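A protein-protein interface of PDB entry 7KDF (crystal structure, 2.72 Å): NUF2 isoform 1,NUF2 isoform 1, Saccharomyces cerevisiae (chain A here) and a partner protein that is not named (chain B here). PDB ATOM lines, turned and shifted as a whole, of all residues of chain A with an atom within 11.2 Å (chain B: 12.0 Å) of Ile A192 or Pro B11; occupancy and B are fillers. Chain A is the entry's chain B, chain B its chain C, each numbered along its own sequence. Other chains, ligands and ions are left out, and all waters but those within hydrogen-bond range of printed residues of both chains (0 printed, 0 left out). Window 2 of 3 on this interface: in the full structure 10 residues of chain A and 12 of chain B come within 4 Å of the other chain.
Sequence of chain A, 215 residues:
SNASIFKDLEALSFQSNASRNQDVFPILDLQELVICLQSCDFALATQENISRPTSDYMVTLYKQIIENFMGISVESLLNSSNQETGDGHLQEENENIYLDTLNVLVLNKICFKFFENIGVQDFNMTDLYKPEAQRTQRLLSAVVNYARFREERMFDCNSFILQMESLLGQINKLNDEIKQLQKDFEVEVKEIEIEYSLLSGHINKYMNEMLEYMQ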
ATOM      1  N   ASP A 184      35.084  13.458   6.178  1.00  0.00           N
ATOM      2  CA  ASP A 184      33.901  12.877   6.805  1.00  0.00           C
ATOM      3  C   ASP A 184      32.668  13.051   5.929  1.00  0.00           C
ATOM      4  O   ASP A 184      31.846  12.135   5.809  1.00  0.00           O
ATOM      5  CB  ASP A 184      33.679  13.509   8.177  1.00  0.00           C
ATOM      6  CG  ASP A 184      34.703  13.062   9.192  1.00  0.00           C
ATOM      7  OD1 ASP A 184      35.544  12.199   8.853  1.00  0.00           O
ATOM      8  OD2 ASP A 184      34.671  13.578  10.329  1.00  0.00           O
ATOM      9  N   PHE A 185      32.520  14.225   5.314  1.00  0.00           N
ATOM     10  CA  PHE A 185      31.392  14.453   4.420  1.00  0.00           C
ATOM     11  C   PHE A 185      31.449  13.525   3.217  1.00  0.00           C
ATOM     12  O   PHE A 185      30.410  13.064   2.729  1.00  0.00           O
ATOM     13  CB  PHE A 185      31.364  15.912   3.974  1.00  0.00           C
ATOM     14  CG  PHE A 185      30.180  16.257   3.123  1.00  0.00           C
ATOM     15  CD1 PHE A 185      30.306  16.373   1.747  1.00  0.00           C
ATOM     16  CD2 PHE A 185      28.930  16.429   3.698  1.00  0.00           C
ATOM     17  CE1 PHE A 185      29.211  16.689   0.963  1.00  0.00           C
ATOM     18  CE2 PHE A 185      27.829  16.738   2.922  1.00  0.00           C
ATOM     19  CZ  PHE A 185      27.967  16.866   1.552  1.00  0.00           C
ATOM     20  N   GLU A 186      32.655  13.242   2.721  1.00  0.00           N
ATOM     21  CA  GLU A 186      32.791  12.307   1.613  1.00  0.00           C
ATOM     22  C   GLU A 186      32.324  10.913   2.015  1.00  0.00           C
ATOM     23  O   GLU A 186      31.734  10.187   1.205  1.00  0.00           O
ATOM     24  CB  GLU A 186      34.239  12.281   1.132  1.00  0.00           C
ATOM     25  CG  GLU A 186      34.513  13.210  -0.038  1.00  0.00           C
ATOM     26  CD  GLU A 186      35.925  13.069  -0.573  1.00  0.00           C
ATOM     27  OE1 GLU A 186      36.567  12.029  -0.302  1.00  0.00           O
ATOM     28  OE2 GLU A 186      36.395  14.001  -1.262  1.00  0.00           O
ATOM     29  N   VAL A 187      32.587  10.519   3.262  1.00  0.00           N
ATOM     30  CA  VAL A 187      32.056   9.259   3.773  1.00  0.00           C
ATOM     31  C   VAL A 187      30.533   9.304   3.815  1.00  0.00           C
ATOM     32  O   VAL A 187      29.856   8.349   3.413  1.00  0.00           O
ATOM     33  CB  VAL A 187      32.656   8.952   5.158  1.00  0.00           C
ATOM     34  CG1 VAL A 187      31.804   7.930   5.904  1.00  0.00           C
ATOM     35  CG2 VAL A 187      34.088   8.464   5.013  1.00  0.00           C
ATOM     36  N   GLU A 188      29.970  10.418   4.298  1.00  0.00           N
ATOM     37  CA  GLU A 188      28.518  10.558   4.329  1.00  0.00           C
ATOM     38  C   GLU A 188      27.928  10.420   2.935  1.00  0.00           C
ATOM     39  O   GLU A 188      26.930   9.716   2.743  1.00  0.00           O
ATOM     40  CB  GLU A 188      28.122  11.909   4.921  1.00  0.00           C
ATOM     41  CG  GLU A 188      28.200  12.010   6.429  1.00  0.00           C
ATOM     42  CD  GLU A 188      27.612  13.314   6.939  1.00  0.00           C
ATOM     43  OE1 GLU A 188      26.633  13.803   6.334  1.00  0.00           O
ATOM     44  OE2 GLU A 188      28.135  13.859   7.933  1.00  0.00           O
ATOM     45  N   VAL A 189      28.545  11.068   1.947  1.00  0.00           N
ATOM     46  CA  VAL A 189      27.999  11.049   0.593  1.00  0.00           C
ATOM     47  C   VAL A 189      27.953   9.626   0.047  1.00  0.00           C
ATOM     48  O   VAL A 189      26.956   9.217  -0.561  1.00  0.00           O
ATOM     49  CB  VAL A 189      28.807  11.983  -0.329  1.00  0.00           C
ATOM     50  CG1 VAL A 189      28.544  11.638  -1.778  1.00  0.00           C
ATOM     51  CG2 VAL A 189      28.455  13.444  -0.068  1.00  0.00           C
ATOM     52  N   LYS A 190      29.019   8.843   0.275  1.00  0.00           N
ATOM     53  CA  LYS A 190      29.142   7.527  -0.346  1.00  0.00           C
ATOM     54  C   LYS A 190      28.163   6.536   0.270  1.00  0.00           C
ATOM     55  O   LYS A 190      27.456   5.826  -0.454  1.00  0.00           O
ATOM     56  CB  LYS A 190      30.594   7.020  -0.270  1.00  0.00           C
ATOM     57  CG  LYS A 190      30.744   5.684  -1.039  1.00  0.00           C
ATOM     58  CD  LYS A 190      30.343   5.990  -2.486  1.00  0.00           C
ATOM     59  CE  LYS A 190      30.528   4.851  -3.484  1.00  0.00           C
ATOM     60  NZ  LYS A 190      30.034   5.197  -4.860  1.00  0.00           N
ATOM     61  N   GLU A 191      28.048   6.529   1.599  1.00  0.00           N
ATOM     62  CA  GLU A 191      27.144   5.584   2.242  1.00  0.00           C
ATOM     63  C   GLU A 191      25.724   5.783   1.742  1.00  0.00           C
ATOM     64  O   GLU A 191      24.993   4.813   1.515  1.00  0.00           O
ATOM     65  CB  GLU A 191      27.231   5.729   3.760  1.00  0.00           C
ATOM     66  CG  GLU A 191      28.614   5.434   4.327  1.00  0.00           C
ATOM     67  CD  GLU A 191      28.639   5.516   5.842  1.00  0.00           C
ATOM     68  OE1 GLU A 191      29.543   4.908   6.456  1.00  0.00           O
ATOM     69  OE2 GLU A 191      27.755   6.192   6.417  1.00  0.00           O
ATOM     70  N   ILE A 192      25.333   7.038   1.521  1.00  0.00           N
ATOM     71  CA  ILE A 192      24.084   7.316   0.828  1.00  0.00           C
ATOM     72  C   ILE A 192      24.148   6.824  -0.614  1.00  0.00           C
ATOM     73  O   ILE A 192      23.198   6.213  -1.116  1.00  0.00           O
ATOM     74  CB  ILE A 192      23.766   8.819   0.905  1.00  0.00           C
ATOM     75  CG1 ILE A 192      23.432   9.206   2.349  1.00  0.00           C
ATOM     76  CG2 ILE A 192      22.631   9.167  -0.045  1.00  0.00           C
ATOM     77  CD1 ILE A 192      23.239  10.693   2.554  1.00  0.00           C
ATOM     78  N   GLU A 193      25.267   7.072  -1.301  1.00  0.00           N
ATOM     79  CA  GLU A 193      25.389   6.643  -2.692  1.00  0.00           C
ATOM     80  C   GLU A 193      25.369   5.123  -2.815  1.00  0.00           C
ATOM     81  O   GLU A 193      24.796   4.580  -3.766  1.00  0.00           O
ATOM     82  CB  GLU A 193      26.663   7.217  -3.313  1.00  0.00           C
ATOM     83  CG  GLU A 193      26.527   8.661  -3.768  1.00  0.00           C
ATOM     84  CD  GLU A 193      25.840   8.791  -5.116  1.00  0.00           C
ATOM     85  OE1 GLU A 193      25.503   7.749  -5.719  1.00  0.00           O
ATOM     86  OE2 GLU A 193      25.639   9.936  -5.576  1.00  0.00           O
ATOM     87  N   ILE A 194      26.004   4.421  -1.875  1.00  0.00           N
ATOM     88  CA  ILE A 194      25.969   2.961  -1.889  1.00  0.00           C
ATOM     89  C   ILE A 194      24.534   2.470  -1.749  1.00  0.00           C
ATOM     90  O   ILE A 194      24.059   1.644  -2.537  1.00  0.00           O
ATOM     91  CB  ILE A 194      26.870   2.392  -0.777  1.00  0.00           C
ATOM     92  CG1 ILE A 194      28.344   2.455  -1.187  1.00  0.00           C
ATOM     93  CG2 ILE A 194      26.466   0.964  -0.434  1.00  0.00           C
ATOM     94  CD1 ILE A 194      28.667   1.657  -2.430  1.00  0.00           C
ATOM     95  N   GLU A 195      23.818   2.991  -0.750  1.00  0.00           N
ATOM     96  CA  GLU A 195      22.453   2.539  -0.500  1.00  0.00           C
ATOM     97  C   GLU A 195      21.534   2.893  -1.660  1.00  0.00           C
ATOM     98  O   GLU A 195      20.664   2.098  -2.035  1.00  0.00           O
ATOM     99  CB  GLU A 195      21.934   3.137   0.807  1.00  0.00           C
ATOM    100  CG  GLU A 195      20.906   2.272   1.519  1.00  0.00           C
ATOM    101  CD  GLU A 195      21.445   0.903   1.885  1.00  0.00           C
ATOM    102  OE1 GLU A 195      20.675  -0.081   1.806  1.00  0.00           O
ATOM    103  OE2 GLU A 195      22.637   0.811   2.251  1.00  0.00           O
ATOM    104  N   TYR A 196      21.709   4.079  -2.244  1.00  0.00           N
ATOM    105  CA  TYR A 196      20.884   4.447  -3.389  1.00  0.00           C
ATOM    106  C   TYR A 196      21.103   3.490  -4.552  1.00  0.00           C
ATOM    107  O   TYR A 196      20.155   3.149  -5.271  1.00  0.00           O
ATOM    108  CB  TYR A 196      21.170   5.880  -3.833  1.00  0.00           C
ATOM    109  CG  TYR A 196      20.568   6.181  -5.186  1.00  0.00           C
ATOM    110  CD1 TYR A 196      19.248   6.599  -5.299  1.00  0.00           C
ATOM    111  CD2 TYR A 196      21.308   6.022  -6.352  1.00  0.00           C
ATOM    112  CE1 TYR A 196      18.685   6.860  -6.534  1.00  0.00           C
ATOM    113  CE2 TYR A 196      20.753   6.278  -7.590  1.00  0.00           C
ATOM    114  CZ  TYR A 196      19.442   6.698  -7.677  1.00  0.00           C
ATOM    115  OH  TYR A 196      18.895   6.957  -8.912  1.00  0.00           O
ATOM    116  N   SER A 197      22.351   3.070  -4.773  1.00  0.00           N
ATOM    117  CA  SER A 197      22.632   2.154  -5.874  1.00  0.00           C
ATOM    118  C   SER A 197      21.901   0.832  -5.689  1.00  0.00           C
ATOM    119  O   SER A 197      21.387   0.259  -6.657  1.00  0.00           O
ATOM    120  CB  SER A 197      24.135   1.926  -6.005  1.00  0.00           C
ATOM    121  OG  SER A 197      24.749   3.014  -6.670  1.00  0.00           O
ATOM    122  N   LEU A 198      21.841   0.334  -4.452  1.00  0.00           N
ATOM    123  CA  LEU A 198      21.055  -0.861  -4.170  1.00  0.00           C
ATOM    124  C   LEU A 198      19.593  -0.645  -4.536  1.00  0.00           C
ATOM    125  O   LEU A 198      18.973  -1.485  -5.200  1.00  0.00           O
ATOM    126  CB  LEU A 198      21.188  -1.237  -2.694  1.00  0.00           C
ATOM    127  CG  LEU A 198      22.572  -1.716  -2.256  1.00  0.00           C
ATOM    128  CD1 LEU A 198      22.578  -2.125  -0.786  1.00  0.00           C
ATOM    129  CD2 LEU A 198      23.030  -2.865  -3.147  1.00  0.00           C
ATOM    130  N   LEU A 199      19.031   0.492  -4.126  1.00  0.00           N
ATOM    131  CA  LEU A 199      17.632   0.775  -4.426  1.00  0.00           C
ATOM    132  C   LEU A 199      17.414   0.963  -5.922  1.00  0.00           C
ATOM    133  O   LEU A 199      16.383   0.544  -6.459  1.00  0.00           O
ATOM    134  CB  LEU A 199      17.172   2.007  -3.649  1.00  0.00           C
ATOM    135  CG  LEU A 199      15.786   2.539  -4.003  1.00  0.00           C
ATOM    136  CD1 LEU A 199      14.732   1.548  -3.558  1.00  0.00           C
ATOM    137  CD2 LEU A 199      15.561   3.877  -3.338  1.00  0.00           C
ATOM    138  N   SER A 200      18.368   1.594  -6.611  1.00  0.00           N
ATOM    139  CA  SER A 200      18.238   1.771  -8.055  1.00  0.00           C
ATOM    140  C   SER A 200      18.223   0.429  -8.773  1.00  0.00           C
ATOM    141  O   SER A 200      17.422   0.217  -9.692  1.00  0.00           O
ATOM    142  CB  SER A 200      19.371   2.646  -8.588  1.00  0.00           C
ATOM    143  OG  SER A 200      19.291   2.765  -9.999  1.00  0.00           O
ATOM    144  N   GLY A 201      19.105  -0.486  -8.371  1.00  0.00           N
ATOM    145  CA  GLY A 201      19.083  -1.819  -8.948  1.00  0.00           C
ATOM    146  C   GLY A 201      17.813  -2.571  -8.609  1.00  0.00           C
ATOM    147  O   GLY A 201      17.287  -3.326  -9.433  1.00  0.00           O
ATOM    148  N   ASP B   5      15.948  19.657  12.740  1.00  0.00           N
ATOM    149  CA  ASP B   5      17.183  19.949  12.023  1.00  0.00           C
ATOM    150  C   ASP B   5      16.936  20.090  10.527  1.00  0.00           C
ATOM    151  O   ASP B   5      17.826  20.506   9.783  1.00  0.00           O
ATOM    152  CB  ASP B   5      18.223  18.855  12.274  1.00  0.00           C
ATOM    153  CG  ASP B   5      19.224  19.235  13.347  1.00  0.00           C
ATOM    154  OD1 ASP B   5      19.149  20.372  13.856  1.00  0.00           O
ATOM    155  OD2 ASP B   5      20.087  18.395  13.679  1.00  0.00           O
ATOM    156  N   ASN B   6      15.722  19.737  10.096  1.00  0.00           N
ATOM    157  CA  ASN B   6      15.350  19.655   8.683  1.00  0.00           C
ATOM    158  C   ASN B   6      16.252  18.697   7.913  1.00  0.00           C
ATOM    159  O   ASN B   6      16.335  18.762   6.681  1.00  0.00           O
ATOM    160  CB  ASN B   6      15.345  21.037   8.018  1.00  0.00           C
ATOM    161  CG  ASN B   6      14.386  21.999   8.690  1.00  0.00           C
ATOM    162  OD1 ASN B   6      14.568  22.367   9.850  1.00  0.00           O
ATOM    163  ND2 ASN B   6      13.354  22.407   7.963  1.00  0.00           N
ATOM    164  N   LEU B   7      16.929  17.812   8.630  1.00  0.00           N
ATOM    165  CA  LEU B   7      17.806  16.805   8.069  1.00  0.00           C
ATOM    166  C   LEU B   7      17.192  15.428   8.283  1.00  0.00           C
ATOM    167  O   LEU B   7      16.040  15.290   8.716  1.00  0.00           O
ATOM    168  CB  LEU B   7      19.195  16.899   8.701  1.00  0.00           C
ATOM    169  CG  LEU B   7      20.089  18.046   8.232  1.00  0.00           C
ATOM    170  CD1 LEU B   7      21.527  17.811   8.669  1.00  0.00           C
ATOM    171  CD2 LEU B   7      20.002  18.218   6.722  1.00  0.00           C
ATOM    172  N   LEU B   8      17.961  14.398   7.967  1.00  0.00           N
ATOM    173  CA  LEU B   8      17.556  13.027   8.206  1.00  0.00           C
ATOM    174  C   LEU B   8      18.393  12.433   9.325  1.00  0.00           C
ATOM    175  O   LEU B   8      19.625  12.408   9.255  1.00  0.00           O
ATOM    176  CB  LEU B   8      17.676  12.184   6.937  1.00  0.00           C
ATOM    177  CG  LEU B   8      16.588  12.480   5.892  1.00  0.00           C
ATOM    178  CD1 LEU B   8      16.508  11.370   4.864  1.00  0.00           C
ATOM    179  CD2 LEU B   8      15.225  12.685   6.559  1.00  0.00           C
ATOM    180  N   ASP B   9      17.698  11.937  10.338  1.00  0.00           N
ATOM    181  CA  ASP B   9      18.304  11.162  11.411  1.00  0.00           C
ATOM    182  C   ASP B   9      19.211  10.063  10.902  1.00  0.00           C
ATOM    183  O   ASP B   9      20.352   9.919  11.337  1.00  0.00           O
ATOM    184  CB  ASP B   9      17.164  10.617  12.250  1.00  0.00           C
ATOM    185  CG  ASP B   9      16.577  11.680  13.142  1.00  0.00           C
ATOM    186  OD1 ASP B   9      17.416  12.418  13.701  1.00  0.00           O
ATOM    187  OD2 ASP B   9      15.332  11.893  13.149  1.00  0.00           O
ATOM    188  N   ASN B  10      18.730   9.270   9.917  1.00  0.00           N
ATOM    189  CA  ASN B  10      19.566   8.256   9.299  1.00  0.00           C
ATOM    190  C   ASN B  10      19.088   8.033   7.854  1.00  0.00           C
ATOM    191  O   ASN B  10      18.238   7.188   7.602  1.00  0.00           O
ATOM    192  CB  ASN B  10      19.561   6.929  10.066  1.00  0.00           C
ATOM    193  CG  ASN B  10      20.766   6.056   9.744  1.00  0.00           C
ATOM    194  OD1 ASN B  10      21.455   6.262   8.744  1.00  0.00           O
ATOM    195  ND2 ASN B  10      21.013   5.059  10.594  1.00  0.00           N
ATOM    196  N   PRO B  11      19.646   8.806   6.924  1.00  0.00           N
ATOM    197  CA  PRO B  11      19.229   8.618   5.515  1.00  0.00           C
ATOM    198  C   PRO B  11      19.603   7.268   4.937  1.00  0.00           C
ATOM    199  O   PRO B  11      18.939   6.815   3.996  1.00  0.00           O
ATOM    200  CB  PRO B  11      19.955   9.762   4.790  1.00  0.00           C
ATOM    201  CG  PRO B  11      21.111  10.097   5.655  1.00  0.00           C
ATOM    202  CD  PRO B  11      20.661   9.848   7.066  1.00  0.00           C
ATOM    203  N   VAL B  12      20.639   6.611   5.460  1.00  0.00           N
ATOM    204  CA  VAL B  12      21.035   5.309   4.931  1.00  0.00           C
ATOM    205  C   VAL B  12      19.988   4.255   5.267  1.00  0.00           C
ATOM    206  O   VAL B  12      19.554   3.491   4.399  1.00  0.00           O
ATOM    207  CB  VAL B  12      22.421   4.911   5.467  1.00  0.00           C
ATOM    208  CG1 VAL B  12      22.789   3.513   4.986  1.00  0.00           C
ATOM    209  CG2 VAL B  12      23.468   5.927   5.044  1.00  0.00           C
ATOM    210  N   GLU B  13      19.568   4.194   6.533  1.00  0.00           N
ATOM    211  CA  GLU B  13      18.487   3.288   6.891  1.00  0.00           C
ATOM    212  C   GLU B  13      17.195   3.695   6.216  1.00  0.00           C
ATOM    213  O   GLU B  13      16.393   2.832   5.849  1.00  0.00           O
ATOM    214  CB  GLU B  13      18.294   3.217   8.410  1.00  0.00           C
ATOM    215  CG  GLU B  13      19.469   2.610   9.137  1.00  0.00           C
ATOM    216  CD  GLU B  13      19.546   1.095   8.969  1.00  0.00           C
ATOM    217  OE1 GLU B  13      18.547   0.400   9.259  1.00  0.00           O
ATOM    218  OE2 GLU B  13      20.600   0.602   8.513  1.00  0.00           O
ATOM    219  N   PHE B  14      16.961   5.001   6.054  1.00  0.00           N
ATOM    220  CA  PHE B  14      15.676   5.417   5.511  1.00  0.00           C
ATOM    221  C   PHE B  14      15.493   4.744   4.155  1.00  0.00           C
ATOM    222  O   PHE B  14      14.496   4.059   3.902  1.00  0.00           O
ATOM    223  CB  PHE B  14      15.616   6.920   5.270  1.00  0.00           C
ATOM    224  CG  PHE B  14      14.232   7.497   5.387  1.00  0.00           C
ATOM    225  CD1 PHE B  14      13.921   8.269   6.479  1.00  0.00           C
ATOM    226  CD2 PHE B  14      13.172   6.961   4.666  1.00  0.00           C
ATOM    227  CE1 PHE B  14      12.658   8.782   6.653  1.00  0.00           C
ATOM    228  CE2 PHE B  14      11.881   7.428   4.852  1.00  0.00           C
ATOM    229  CZ  PHE B  14      11.627   8.336   5.856  1.00  0.00           C
ATOM    230  N   LEU B  15      16.506   4.902   3.288  1.00  0.00           N
ATOM    231  CA  LEU B  15      16.502   4.320   1.948  1.00  0.00           C
ATOM    232  C   LEU B  15      16.450   2.803   1.998  1.00  0.00           C
ATOM    233  O   LEU B  15      15.742   2.166   1.208  1.00  0.00           O
ATOM    234  CB  LEU B  15      17.754   4.754   1.184  1.00  0.00           C
ATOM    235  CG  LEU B  15      17.869   6.167   0.622  1.00  0.00           C
ATOM    236  CD1 LEU B  15      19.285   6.420   0.133  1.00  0.00           C
ATOM    237  CD2 LEU B  15      16.886   6.331  -0.519  1.00  0.00           C
ATOM    238  N   LYS B  16      17.226   2.208   2.900  1.00  0.00           N
ATOM    239  CA  LYS B  16      17.247   0.758   3.041  1.00  0.00           C
ATOM    240  C   LYS B  16      15.850   0.214   3.341  1.00  0.00           C
ATOM    241  O   LYS B  16      15.394  -0.747   2.708  1.00  0.00           O
ATOM    242  CB  LYS B  16      18.229   0.380   4.145  1.00  0.00           C
ATOM    243  CG  LYS B  16      18.365  -1.105   4.358  1.00  0.00           C
ATOM    244  CD  LYS B  16      19.301  -1.365   5.521  1.00  0.00           C
ATOM    245  CE  LYS B  16      19.375  -2.850   5.847  1.00  0.00           C
ATOM    246  NZ  LYS B  16      20.344  -3.031   6.958  1.00  0.00           N
ATOM    247  N   GLU B  17      15.139   0.854   4.277  1.00  0.00           N
ATOM    248  CA  GLU B  17      13.780   0.429   4.616  1.00  0.00           C
ATOM    249  C   GLU B  17      12.855   0.452   3.402  1.00  0.00           C
ATOM    250  O   GLU B  17      12.015  -0.443   3.234  1.00  0.00           O
ATOM    251  CB  GLU B  17      13.220   1.318   5.725  1.00  0.00           C
ATOM    252  CG  GLU B  17      14.022   1.260   7.010  1.00  0.00           C
ATOM    253  CD  GLU B  17      13.564   2.281   8.022  1.00  0.00           C
ATOM    254  OE1 GLU B  17      14.245   2.445   9.058  1.00  0.00           O
ATOM    255  OE2 GLU B  17      12.518   2.918   7.777  1.00  0.00           O
ATOM    256  N   VAL B  18      12.983   1.471   2.552  1.00  0.00           N
ATOM    257  CA  VAL B  18      12.113   1.564   1.384  1.00  0.00           C
ATOM    258  C   VAL B  18      12.386   0.402   0.439  1.00  0.00           C
ATOM    259  O   VAL B  18      11.459  -0.212  -0.105  1.00  0.00           O
ATOM    260  CB  VAL B  18      12.312   2.918   0.683  1.00  0.00           C
ATOM    261  CG1 VAL B  18      11.354   3.049  -0.489  1.00  0.00           C
ATOM    262  CG2 VAL B  18      12.179   4.051   1.668  1.00  0.00           C
ATOM    263  N   ARG B  19      13.666   0.083   0.228  1.00  0.00           N
ATOM    264  CA  ARG B  19      14.024  -1.053  -0.615  1.00  0.00           C
ATOM    265  C   ARG B  19      13.509  -2.361  -0.028  1.00  0.00           C
ATOM    266  O   ARG B  19      13.040  -3.239  -0.762  1.00  0.00           O
ATOM    267  CB  ARG B  19      15.541  -1.113  -0.795  1.00  0.00           C
ATOM    268  CG  ARG B  19      16.033  -2.357  -1.512  1.00  0.00           C
ATOM    269  CD  ARG B  19      17.522  -2.276  -1.825  1.00  0.00           C
ATOM    270  NE  ARG B  19      18.325  -2.018  -0.633  1.00  0.00           N
ATOM    271  CZ  ARG B  19      18.838  -2.966   0.144  1.00  0.00           C
ATOM    272  NH1 ARG B  19      18.634  -4.246  -0.143  1.00  0.00           N
ATOM    273  NH2 ARG B  19      19.555  -2.636   1.210  1.00  0.00           N
ATOM    274  N   GLU B  20      13.596  -2.513   1.295  1.00  0.00           N
ATOM    275  CA  GLU B  20      13.158  -3.753   1.925  1.00  0.00           C
ATOM    276  C   GLU B  20      11.640  -3.867   1.986  1.00  0.00           C
ATOM    277  O   GLU B  20      11.120  -4.976   2.142  1.00  0.00           O
ATOM    278  CB  GLU B  20      13.774  -3.860   3.320  1.00  0.00           C
ATOM    279  CG  GLU B  20      15.291  -3.992   3.277  1.00  0.00           C
ATOM    280  CD  GLU B  20      15.907  -4.270   4.632  1.00  0.00           C
ATOM    281  OE1 GLU B  20      15.300  -3.890   5.657  1.00  0.00           O
ATOM    282  OE2 GLU B  20      17.006  -4.865   4.668  1.00  0.00           O
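Among the printed residues, pairs that only touch across the chains: Glu A191 with Val B12 (3.98 Å), Ile A192 with Pro B11 (3.8 Å), Glu A195 with Val B12 (3.4 Å), Glu A195 with Lys B16 (3.4 Å), Leu A198 with Arg B19 (3.6 Å), Leu A199 with Leu B15 (3.97 Å) and Leu A199 with Arg B19 (3.9 Å).
No residue of chain B comes within 4 Å of Glu A188.
No residue of chain B comes within 4 Å of Val A189.
No residue of chain B comes within 4 Å of Lys A190.
Ile A192 touches one residue of chain B.
Of the printed residues of chain A, Lys B16 touches Glu A195.
Val B18 touches none of the printed residues of chain A.
Of the printed residues of chain A, Arg B19 touches Glu A195, Leu A198 and Leu A199.
The backbone NH (N) of Val B12 sits close to the side-chain amide oxygen (OD1) of Asn B10 (3.4 Å).
The side-chain amino group (NZ) of Lys B16 lies within salt-bridge range of the side-chain carboxylate (OE2) of Glu B13.
The side-chain carboxylate (OE1) of Glu A195 lies within salt-bridge range of the guanidinium group (NH2) of Arg B19, 2.9 Å away.
Of the 16 printed residues of chain B, 5 touch a printed residue of chain A.
Among the printed residues, 8 pairs touch across the chains.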
